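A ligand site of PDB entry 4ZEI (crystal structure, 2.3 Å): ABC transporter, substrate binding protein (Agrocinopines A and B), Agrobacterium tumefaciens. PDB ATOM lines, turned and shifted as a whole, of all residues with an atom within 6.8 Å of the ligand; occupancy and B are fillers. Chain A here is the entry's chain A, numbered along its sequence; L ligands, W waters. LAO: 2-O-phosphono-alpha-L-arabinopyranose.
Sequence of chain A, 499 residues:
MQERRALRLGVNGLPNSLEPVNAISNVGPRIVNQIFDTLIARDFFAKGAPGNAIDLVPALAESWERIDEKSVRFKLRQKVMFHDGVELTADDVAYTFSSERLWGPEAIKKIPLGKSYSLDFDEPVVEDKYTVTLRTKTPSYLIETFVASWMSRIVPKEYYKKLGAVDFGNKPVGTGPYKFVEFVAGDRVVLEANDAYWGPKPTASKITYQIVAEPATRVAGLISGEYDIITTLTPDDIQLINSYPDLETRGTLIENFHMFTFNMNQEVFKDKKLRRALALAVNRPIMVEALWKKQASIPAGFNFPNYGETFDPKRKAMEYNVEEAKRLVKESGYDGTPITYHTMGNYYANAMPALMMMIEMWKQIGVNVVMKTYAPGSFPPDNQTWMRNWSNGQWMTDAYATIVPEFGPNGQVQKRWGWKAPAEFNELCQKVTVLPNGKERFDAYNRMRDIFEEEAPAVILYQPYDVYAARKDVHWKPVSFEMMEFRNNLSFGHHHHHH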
ATOM      1  N   ILE A  24      -7.617 -17.893   5.182  1.00  0.00           N
ATOM      2  CA  ILE A  24      -6.459 -17.872   4.260  1.00  0.00           C
ATOM      3  C   ILE A  24      -5.852 -19.294   4.163  1.00  0.00           C
ATOM      4  O   ILE A  24      -5.345 -19.833   5.146  1.00  0.00           O
ATOM      5  CB  ILE A  24      -5.435 -16.738   4.578  1.00  0.00           C
ATOM      6  CG1 ILE A  24      -6.005 -15.378   4.141  1.00  0.00           C
ATOM      7  CG2 ILE A  24      -4.076 -17.000   3.902  1.00  0.00           C
ATOM      8  CD1 ILE A  24      -5.565 -14.258   4.892  1.00  0.00           C
ATOM      9  N   SER A  25      -6.061 -19.904   2.991  1.00  0.00           N
ATOM     10  CA  SER A  25      -5.683 -21.258   2.603  1.00  0.00           C
ATOM     11  C   SER A  25      -5.987 -21.445   1.111  1.00  0.00           C
ATOM     12  O   SER A  25      -6.409 -20.491   0.458  1.00  0.00           O
ATOM     13  CB  SER A  25      -6.455 -22.294   3.423  1.00  0.00           C
ATOM     14  OG  SER A  25      -7.859 -22.135   3.352  1.00  0.00           O
ATOM     15  N   ASN A  26      -5.785 -22.661   0.569  1.00  0.00           N
ATOM     16  CA  ASN A  26      -6.087 -22.999  -0.821  1.00  0.00           C
ATOM     17  C   ASN A  26      -7.604 -23.204  -0.969  1.00  0.00           C
ATOM     18  O   ASN A  26      -8.126 -23.224  -2.101  1.00  0.00           O
ATOM     19  CB  ASN A  26      -5.406 -24.332  -1.201  1.00  0.00           C
ATOM     20  CG  ASN A  26      -3.914 -24.307  -1.424  1.00  0.00           C
ATOM     21  OD1 ASN A  26      -3.207 -23.313  -1.215  1.00  0.00           O
ATOM     22  ND2 ASN A  26      -3.390 -25.449  -1.855  1.00  0.00           N
ATOM     23  N   VAL A  27      -8.289 -23.421   0.179  1.00  0.00           N
ATOM     24  CA  VAL A  27      -9.709 -23.808   0.249  1.00  0.00           C
ATOM     25  C   VAL A  27     -10.713 -22.767   0.792  1.00  0.00           C
ATOM     26  O   VAL A  27     -11.915 -22.925   0.572  1.00  0.00           O
ATOM     27  CB  VAL A  27      -9.873 -25.196   0.934  1.00  0.00           C
ATOM     28  CG1 VAL A  27      -9.184 -26.290   0.123  1.00  0.00           C
ATOM     29  CG2 VAL A  27      -9.363 -25.174   2.372  1.00  0.00           C
ATOM     30  N   LEU A 113      -2.607 -15.466  12.932  1.00  0.00           N
ATOM     31  CA  LEU A 113      -1.639 -14.948  11.964  1.00  0.00           C
ATOM     32  C   LEU A 113      -1.871 -13.479  11.532  1.00  0.00           C
ATOM     33  O   LEU A 113      -1.194 -12.997  10.612  1.00  0.00           O
ATOM     34  CB  LEU A 113      -1.482 -15.906  10.763  1.00  0.00           C
ATOM     35  CG  LEU A 113      -0.861 -17.270  11.086  1.00  0.00           C
ATOM     36  CD1 LEU A 113      -1.290 -18.317  10.128  1.00  0.00           C
ATOM     37  CD2 LEU A 113       0.653 -17.192  11.184  1.00  0.00           C
ATOM     38  N   TYR A 117       1.005 -11.494   9.418  1.00  0.00           N
ATOM     39  CA  TYR A 117       0.612 -11.247   8.026  1.00  0.00           C
ATOM     40  C   TYR A 117       0.309  -9.761   7.753  1.00  0.00           C
ATOM     41  O   TYR A 117       0.158  -9.372   6.603  1.00  0.00           O
ATOM     42  CB  TYR A 117      -0.603 -12.099   7.636  1.00  0.00           C
ATOM     43  CG  TYR A 117      -0.416 -13.608   7.529  1.00  0.00           C
ATOM     44  CD1 TYR A 117       0.827 -14.187   7.761  1.00  0.00           C
ATOM     45  CD2 TYR A 117      -1.477 -14.439   7.185  1.00  0.00           C
ATOM     46  CE1 TYR A 117       1.004 -15.571   7.657  1.00  0.00           C
ATOM     47  CE2 TYR A 117      -1.302 -15.811   7.039  1.00  0.00           C
ATOM     48  CZ  TYR A 117      -0.062 -16.377   7.275  1.00  0.00           C
ATOM     49  OH  TYR A 117       0.111 -17.735   7.133  1.00  0.00           O
ATOM     50  N   TRP A 150      -6.433 -10.858   0.229  1.00  0.00           N
ATOM     51  CA  TRP A 150      -7.228 -11.761   1.067  1.00  0.00           C
ATOM     52  C   TRP A 150      -7.131 -11.444   2.585  1.00  0.00           C
ATOM     53  O   TRP A 150      -7.830 -12.059   3.397  1.00  0.00           O
ATOM     54  CB  TRP A 150      -6.851 -13.238   0.790  1.00  0.00           C
ATOM     55  CG  TRP A 150      -5.393 -13.621   0.931  1.00  0.00           C
ATOM     56  CD1 TRP A 150      -4.374 -12.866   1.432  1.00  0.00           C
ATOM     57  CD2 TRP A 150      -4.831 -14.902   0.625  1.00  0.00           C
ATOM     58  NE1 TRP A 150      -3.208 -13.584   1.456  1.00  0.00           N
ATOM     59  CE2 TRP A 150      -3.456 -14.834   0.940  1.00  0.00           C
ATOM     60  CE3 TRP A 150      -5.348 -16.099   0.116  1.00  0.00           C
ATOM     61  CZ2 TRP A 150      -2.591 -15.918   0.745  1.00  0.00           C
ATOM     62  CZ3 TRP A 150      -4.491 -17.161  -0.103  1.00  0.00           C
ATOM     63  CH2 TRP A 150      -3.117 -17.062   0.206  1.00  0.00           C
ATOM     64  N   ASN A 256       0.959 -19.174  -6.613  1.00  0.00           N
ATOM     65  CA  ASN A 256       1.172 -19.988  -5.412  1.00  0.00           C
ATOM     66  C   ASN A 256       2.284 -21.017  -5.708  1.00  0.00           C
ATOM     67  O   ASN A 256       2.493 -21.387  -6.859  1.00  0.00           O
ATOM     68  CB  ASN A 256      -0.155 -20.680  -4.992  1.00  0.00           C
ATOM     69  CG  ASN A 256      -0.056 -21.779  -3.954  1.00  0.00           C
ATOM     70  OD1 ASN A 256       0.350 -22.914  -4.242  1.00  0.00           O
ATOM     71  ND2 ASN A 256      -0.502 -21.518  -2.740  1.00  0.00           N
ATOM     72  N   PHE A 257       2.978 -21.461  -4.666  1.00  0.00           N
ATOM     73  CA  PHE A 257       4.002 -22.479  -4.814  1.00  0.00           C
ATOM     74  C   PHE A 257       3.819 -23.621  -3.826  1.00  0.00           C
ATOM     75  O   PHE A 257       3.494 -23.375  -2.659  1.00  0.00           O
ATOM     76  CB  PHE A 257       5.441 -21.884  -4.783  1.00  0.00           C
ATOM     77  CG  PHE A 257       5.989 -21.463  -3.440  1.00  0.00           C
ATOM     78  CD1 PHE A 257       6.555 -22.390  -2.576  1.00  0.00           C
ATOM     79  CD2 PHE A 257       6.001 -20.123  -3.066  1.00  0.00           C
ATOM     80  CE1 PHE A 257       7.063 -22.000  -1.340  1.00  0.00           C
ATOM     81  CE2 PHE A 257       6.553 -19.722  -1.850  1.00  0.00           C
ATOM     82  CZ  PHE A 257       7.057 -20.667  -0.978  1.00  0.00           C
ATOM     83  N   TYR A 347      -4.956 -33.085  -0.512  1.00  0.00           N
ATOM     84  CA  TYR A 347      -5.372 -31.692  -0.268  1.00  0.00           C
ATOM     85  C   TYR A 347      -4.646 -30.801  -1.286  1.00  0.00           C
ATOM     86  O   TYR A 347      -5.232 -29.855  -1.809  1.00  0.00           O
ATOM     87  CB  TYR A 347      -5.046 -31.279   1.181  1.00  0.00           C
ATOM     88  CG  TYR A 347      -5.329 -29.822   1.512  1.00  0.00           C
ATOM     89  CD1 TYR A 347      -6.572 -29.435   1.998  1.00  0.00           C
ATOM     90  CD2 TYR A 347      -4.331 -28.859   1.408  1.00  0.00           C
ATOM     91  CE1 TYR A 347      -6.827 -28.110   2.335  1.00  0.00           C
ATOM     92  CE2 TYR A 347      -4.592 -27.526   1.717  1.00  0.00           C
ATOM     93  CZ  TYR A 347      -5.841 -27.149   2.184  1.00  0.00           C
ATOM     94  OH  TYR A 347      -6.097 -25.851   2.534  1.00  0.00           O
ATOM     95  N   TYR A 348      -3.366 -31.127  -1.544  1.00  0.00           N
ATOM     96  CA  TYR A 348      -2.548 -30.503  -2.576  1.00  0.00           C
ATOM     97  C   TYR A 348      -2.571 -31.486  -3.722  1.00  0.00           C
ATOM     98  O   TYR A 348      -2.434 -32.687  -3.494  1.00  0.00           O
ATOM     99  CB  TYR A 348      -1.090 -30.248  -2.112  1.00  0.00           C
ATOM    100  CG  TYR A 348      -0.979 -29.330  -0.913  1.00  0.00           C
ATOM    101  CD1 TYR A 348      -1.323 -27.979  -1.010  1.00  0.00           C
ATOM    102  CD2 TYR A 348      -0.529 -29.801   0.309  1.00  0.00           C
ATOM    103  CE1 TYR A 348      -1.263 -27.138   0.103  1.00  0.00           C
ATOM    104  CE2 TYR A 348      -0.438 -28.962   1.418  1.00  0.00           C
ATOM    105  CZ  TYR A 348      -0.807 -27.631   1.303  1.00  0.00           C
ATOM    106  OH  TYR A 348      -0.712 -26.811   2.400  1.00  0.00           O
ATOM    107  N   ASN A 389       4.147 -31.236   4.167  1.00  0.00           N
ATOM    108  CA  ASN A 389       3.965 -30.424   2.962  1.00  0.00           C
ATOM    109  C   ASN A 389       3.171 -29.157   3.318  1.00  0.00           C
ATOM    110  O   ASN A 389       2.525 -29.101   4.366  1.00  0.00           O
ATOM    111  CB  ASN A 389       3.341 -31.205   1.791  1.00  0.00           C
ATOM    112  CG  ASN A 389       2.011 -31.882   2.042  1.00  0.00           C
ATOM    113  OD1 ASN A 389       1.228 -31.520   2.937  1.00  0.00           O
ATOM    114  ND2 ASN A 389       1.706 -32.851   1.219  1.00  0.00           N
ATOM    115  N   TRP A 390       3.270 -28.131   2.452  1.00  0.00           N
ATOM    116  CA  TRP A 390       2.608 -26.837   2.626  1.00  0.00           C
ATOM    117  C   TRP A 390       2.575 -26.134   1.258  1.00  0.00           C
ATOM    118  O   TRP A 390       2.985 -26.721   0.262  1.00  0.00           O
ATOM    119  CB  TRP A 390       3.382 -26.016   3.683  1.00  0.00           C
ATOM    120  CG  TRP A 390       2.724 -24.759   4.199  1.00  0.00           C
ATOM    121  CD1 TRP A 390       1.382 -24.473   4.247  1.00  0.00           C
ATOM    122  CD2 TRP A 390       3.395 -23.645   4.795  1.00  0.00           C
ATOM    123  NE1 TRP A 390       1.186 -23.230   4.799  1.00  0.00           N
ATOM    124  CE2 TRP A 390       2.400 -22.701   5.150  1.00  0.00           C
ATOM    125  CE3 TRP A 390       4.741 -23.342   5.062  1.00  0.00           C
ATOM    126  CZ2 TRP A 390       2.722 -21.493   5.784  1.00  0.00           C
ATOM    127  CZ3 TRP A 390       5.058 -22.139   5.664  1.00  0.00           C
ATOM    128  CH2 TRP A 390       4.046 -21.228   6.020  1.00  0.00           C
ATOM    129  N   SER A 391       2.040 -24.925   1.205  1.00  0.00           N
ATOM    130  CA  SER A 391       1.963 -24.060   0.019  1.00  0.00           C
ATOM    131  C   SER A 391       1.926 -22.614   0.511  1.00  0.00           C
ATOM    132  O   SER A 391       1.594 -22.373   1.668  1.00  0.00           O
ATOM    133  CB  SER A 391       0.756 -24.387  -0.859  1.00  0.00           C
ATOM    134  OG  SER A 391      -0.431 -23.668  -0.533  1.00  0.00           O
ATOM    135  N   ASN A 392       2.309 -21.677  -0.364  1.00  0.00           N
ATOM    136  CA  ASN A 392       2.297 -20.251  -0.062  1.00  0.00           C
ATOM    137  C   ASN A 392       1.782 -19.497  -1.262  1.00  0.00           C
ATOM    138  O   ASN A 392       2.311 -19.625  -2.366  1.00  0.00           O
ATOM    139  CB  ASN A 392       3.700 -19.745   0.318  1.00  0.00           C
ATOM    140  CG  ASN A 392       4.064 -19.751   1.785  1.00  0.00           C
ATOM    141  OD1 ASN A 392       3.385 -20.323   2.637  1.00  0.00           O
ATOM    142  ND2 ASN A 392       5.170 -19.123   2.130  1.00  0.00           N
ATOM    143  N   GLY A 393       0.721 -18.722  -1.041  1.00  0.00           N
ATOM    144  CA  GLY A 393       0.118 -17.876  -2.065  1.00  0.00           C
ATOM    145  C   GLY A 393       0.802 -16.535  -2.099  1.00  0.00           C
ATOM    146  O   GLY A 393       0.960 -15.899  -1.054  1.00  0.00           O
ATOM    147  N   GLN A 394       1.246 -16.110  -3.291  1.00  0.00           N
ATOM    148  CA  GLN A 394       1.940 -14.834  -3.473  1.00  0.00           C
ATOM    149  C   GLN A 394       0.905 -13.724  -3.649  1.00  0.00           C
ATOM    150  O   GLN A 394       0.574 -13.314  -4.768  1.00  0.00           O
ATOM    151  CB  GLN A 394       2.972 -14.942  -4.607  1.00  0.00           C
ATOM    152  CG  GLN A 394       3.944 -16.137  -4.446  1.00  0.00           C
ATOM    153  CD  GLN A 394       4.616 -16.205  -3.087  1.00  0.00           C
ATOM    154  OE1 GLN A 394       4.417 -17.146  -2.321  1.00  0.00           O
ATOM    155  NE2 GLN A 394       5.437 -15.224  -2.768  1.00  0.00           N
ATOM    156  N   TRP A 395       0.357 -13.291  -2.500  1.00  0.00           N
ATOM    157  CA  TRP A 395      -0.740 -12.335  -2.322  1.00  0.00           C
ATOM    158  C   TRP A 395      -0.510 -10.844  -2.497  1.00  0.00           C
ATOM    159  O   TRP A 395      -1.449 -10.057  -2.336  1.00  0.00           O
ATOM    160  CB  TRP A 395      -1.459 -12.624  -1.008  1.00  0.00           C
ATOM    161  CG  TRP A 395      -0.591 -12.569   0.226  1.00  0.00           C
ATOM    162  CD1 TRP A 395       0.155 -13.580   0.736  1.00  0.00           C
ATOM    163  CD2 TRP A 395      -0.550 -11.512   1.188  1.00  0.00           C
ATOM    164  NE1 TRP A 395       0.700 -13.207   1.942  1.00  0.00           N
ATOM    165  CE2 TRP A 395       0.283 -11.934   2.237  1.00  0.00           C
ATOM    166  CE3 TRP A 395      -1.109 -10.227   1.240  1.00  0.00           C
ATOM    167  CZ2 TRP A 395       0.558 -11.127   3.356  1.00  0.00           C
ATOM    168  CZ3 TRP A 395      -0.873  -9.441   2.362  1.00  0.00           C
ATOM    169  CH2 TRP A 395      -0.025  -9.884   3.390  1.00  0.00           C
ATOM    170  N   THR A 402       5.599 -14.065   0.128  1.00  0.00           N
ATOM    171  CA  THR A 402       5.375 -14.493   1.517  1.00  0.00           C
ATOM    172  C   THR A 402       6.661 -14.606   2.353  1.00  0.00           C
ATOM    173  O   THR A 402       6.575 -14.993   3.521  1.00  0.00           O
ATOM    174  CB  THR A 402       4.634 -15.835   1.527  1.00  0.00           C
ATOM    175  OG1 THR A 402       5.231 -16.709   0.571  1.00  0.00           O
ATOM    176  CG2 THR A 402       3.138 -15.698   1.299  1.00  0.00           C
ATOM    177  N   GLU A 406       5.776 -15.012   6.341  1.00  0.00           N
ATOM    178  CA  GLU A 406       5.960 -16.428   6.678  1.00  0.00           C
ATOM    179  C   GLU A 406       7.319 -16.778   7.252  1.00  0.00           C
ATOM    180  O   GLU A 406       7.382 -17.467   8.276  1.00  0.00           O
ATOM    181  CB  GLU A 406       5.635 -17.342   5.479  1.00  0.00           C
ATOM    182  CG  GLU A 406       4.227 -17.179   4.911  1.00  0.00           C
ATOM    183  CD  GLU A 406       3.049 -17.720   5.698  1.00  0.00           C
ATOM    184  OE1 GLU A 406       3.234 -18.165   6.850  1.00  0.00           O
ATOM    185  OE2 GLU A 406       1.931 -17.667   5.146  1.00  0.00           O
ATOM    186  N   GLN A 412       5.601 -17.444  11.622  1.00  0.00           N
ATOM    187  CA  GLN A 412       5.444 -18.789  12.194  1.00  0.00           C
ATOM    188  C   GLN A 412       6.597 -19.756  11.931  1.00  0.00           C
ATOM    189  O   GLN A 412       6.830 -20.630  12.755  1.00  0.00           O
ATOM    190  CB  GLN A 412       4.082 -19.387  11.790  1.00  0.00           C
ATOM    191  CG  GLN A 412       3.909 -19.656  10.276  1.00  0.00           C
ATOM    192  CD  GLN A 412       2.588 -20.316   9.948  1.00  0.00           C
ATOM    193  OE1 GLN A 412       1.862 -19.889   9.045  1.00  0.00           O
ATOM    194  NE2 GLN A 412       2.258 -21.402  10.647  1.00  0.00           N
ATOM    195  N   GLU A 482      -5.428 -18.822  -5.860  1.00  0.00           N
ATOM    196  CA  GLU A 482      -6.146 -19.874  -5.112  1.00  0.00           C
ATOM    197  C   GLU A 482      -7.584 -19.445  -4.747  1.00  0.00           C
ATOM    198  O   GLU A 482      -7.971 -19.493  -3.566  1.00  0.00           O
ATOM    199  CB  GLU A 482      -5.465 -20.166  -3.773  1.00  0.00           C
ATOM    200  CG  GLU A 482      -4.035 -20.598  -3.796  1.00  0.00           C
ATOM    201  CD  GLU A 482      -3.317 -19.887  -2.670  1.00  0.00           C
ATOM    202  OE1 GLU A 482      -2.521 -18.987  -2.990  1.00  0.00           O
ATOM    203  OE2 GLU A 482      -3.607 -20.171  -1.484  1.00  0.00           O
HETATM  204  OP2 LAO L   1      -3.885 -24.363   2.142  1.00  0.00           O
HETATM  205  P   LAO L   1      -2.559 -23.756   2.694  1.00  0.00           P
HETATM  206  OP1 LAO L   1      -1.358 -24.352   1.951  1.00  0.00           O
HETATM  207  OP3 LAO L   1      -2.492 -24.082   4.184  1.00  0.00           O
HETATM  208  O2  LAO L   1      -2.604 -22.185   2.489  1.00  0.00           O
HETATM  209  C2  LAO L   1      -1.505 -21.262   2.576  1.00  0.00           C
HETATM  210  C3  LAO L   1      -1.528 -20.594   3.830  1.00  0.00           C
HETATM  211  O3  LAO L   1      -1.278 -21.506   4.975  1.00  0.00           O
HETATM  212  C4  LAO L   1      -0.662 -19.471   3.948  1.00  0.00           C
HETATM  213  O4  LAO L   1       0.691 -19.914   4.076  1.00  0.00           O
HETATM  214  C5  LAO L   1      -0.729 -18.506   2.780  1.00  0.00           C
HETATM  215  O5  LAO L   1      -0.741 -19.171   1.552  1.00  0.00           O
HETATM  216  C1  LAO L   1      -1.667 -20.236   1.460  1.00  0.00           C
HETATM  217  O1  LAO L   1      -1.633 -20.768   0.207  1.00  0.00           O
HETATM  218  O   HOH W   1      -1.154 -19.983   7.307  1.00  0.00           O
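CG2 of Ile 24 touches C5 of the ligand, 3.8 Å away.
CA of Ser 25 touches O2 of the ligand (3.2 Å).
Tyr 117 touches the ligand.
Trp 150 touches the ligand (CH2 to O5, 3.5 Å).
Hydrophobic or aromatic side chains within 4 Å of the ligand: Ile 24, Trp 150, Tyr 347, Tyr 348 and Trp 390.
The nearest printed residue that does not touch the ligand is Val 27 (4.9 Å).
O of Asn 392 sits close to ND2 of Asn 256 (3.4 Å).
The side-chain hydroxyl of Ser 25 lies close to the backbone NH of Val 27, 3.5 Å away.
OH of Tyr 117 lies within hydrogen-bond range of OE1 of Gln 412 (3.4 Å).
The side-chain amide oxygen of Gln 412 lies close to the side-chain carboxylate of Glu 406.
OE2 of Glu 482 lies close to OD1 of Asn 26.
The side-chain amide nitrogen of Asn 392 is in hydrogen-bond range of the side-chain hydroxyl of Thr 402, at 2.9 Å.
OE1 of Gln 394 sits close to O of Asn 392 (3.3 Å).
The side-chain carboxylate (OE2) of Glu 406 sits at hydrogen-bond distance from the side-chain hydroxyl (OH) of Tyr 117 (2.7 Å).
An oxygen (OP1) of the ligand is in hydrogen-bond range of the side-chain hydroxyl (OH) of Tyr 348 (2.6 Å).
The side-chain amide nitrogen (ND2) of Asn 256 is in hydrogen-bond range of an oxygen (O1) of the ligand (3.2 Å).
O5 of the ligand is in hydrogen-bond range of N of Gly 393, at 3.0 Å.
The side-chain carboxylate of Glu 482 sits at hydrogen-bond distance from an oxygen (O1) of the ligand (2.7 Å).
O3 of the ligand lies within hydrogen-bond range of NE1 of Trp 390 (3.0 Å).
OD1 of Asn 26 lies within hydrogen-bond range of O1 of the ligand.
N of Asn 26 is in hydrogen-bond range of OP2 of the ligand, 3.0 Å away.
The side-chain carboxylate (OE2) of Glu 406 is in hydrogen-bond range of an oxygen (O4) of the ligand (2.8 Å).
OD1 of Asn 392 sits at hydrogen-bond distance from O4 of the ligand, at 3.1 Å.
The side-chain hydroxyl (OG) of Ser 391 sits at hydrogen-bond distance from an oxygen (OP1) of the ligand (2.7 Å).
The side-chain hydroxyl (OH) of Tyr 347 is in hydrogen-bond range of an oxygen (OP2) of the ligand, at 2.7 Å.
Water W1 lies within hydrogen-bond range of OH of Tyr 117 (2.6 Å), O3 of the ligand (2.8 Å) and OE1 of Gln 412 (3.5 Å).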
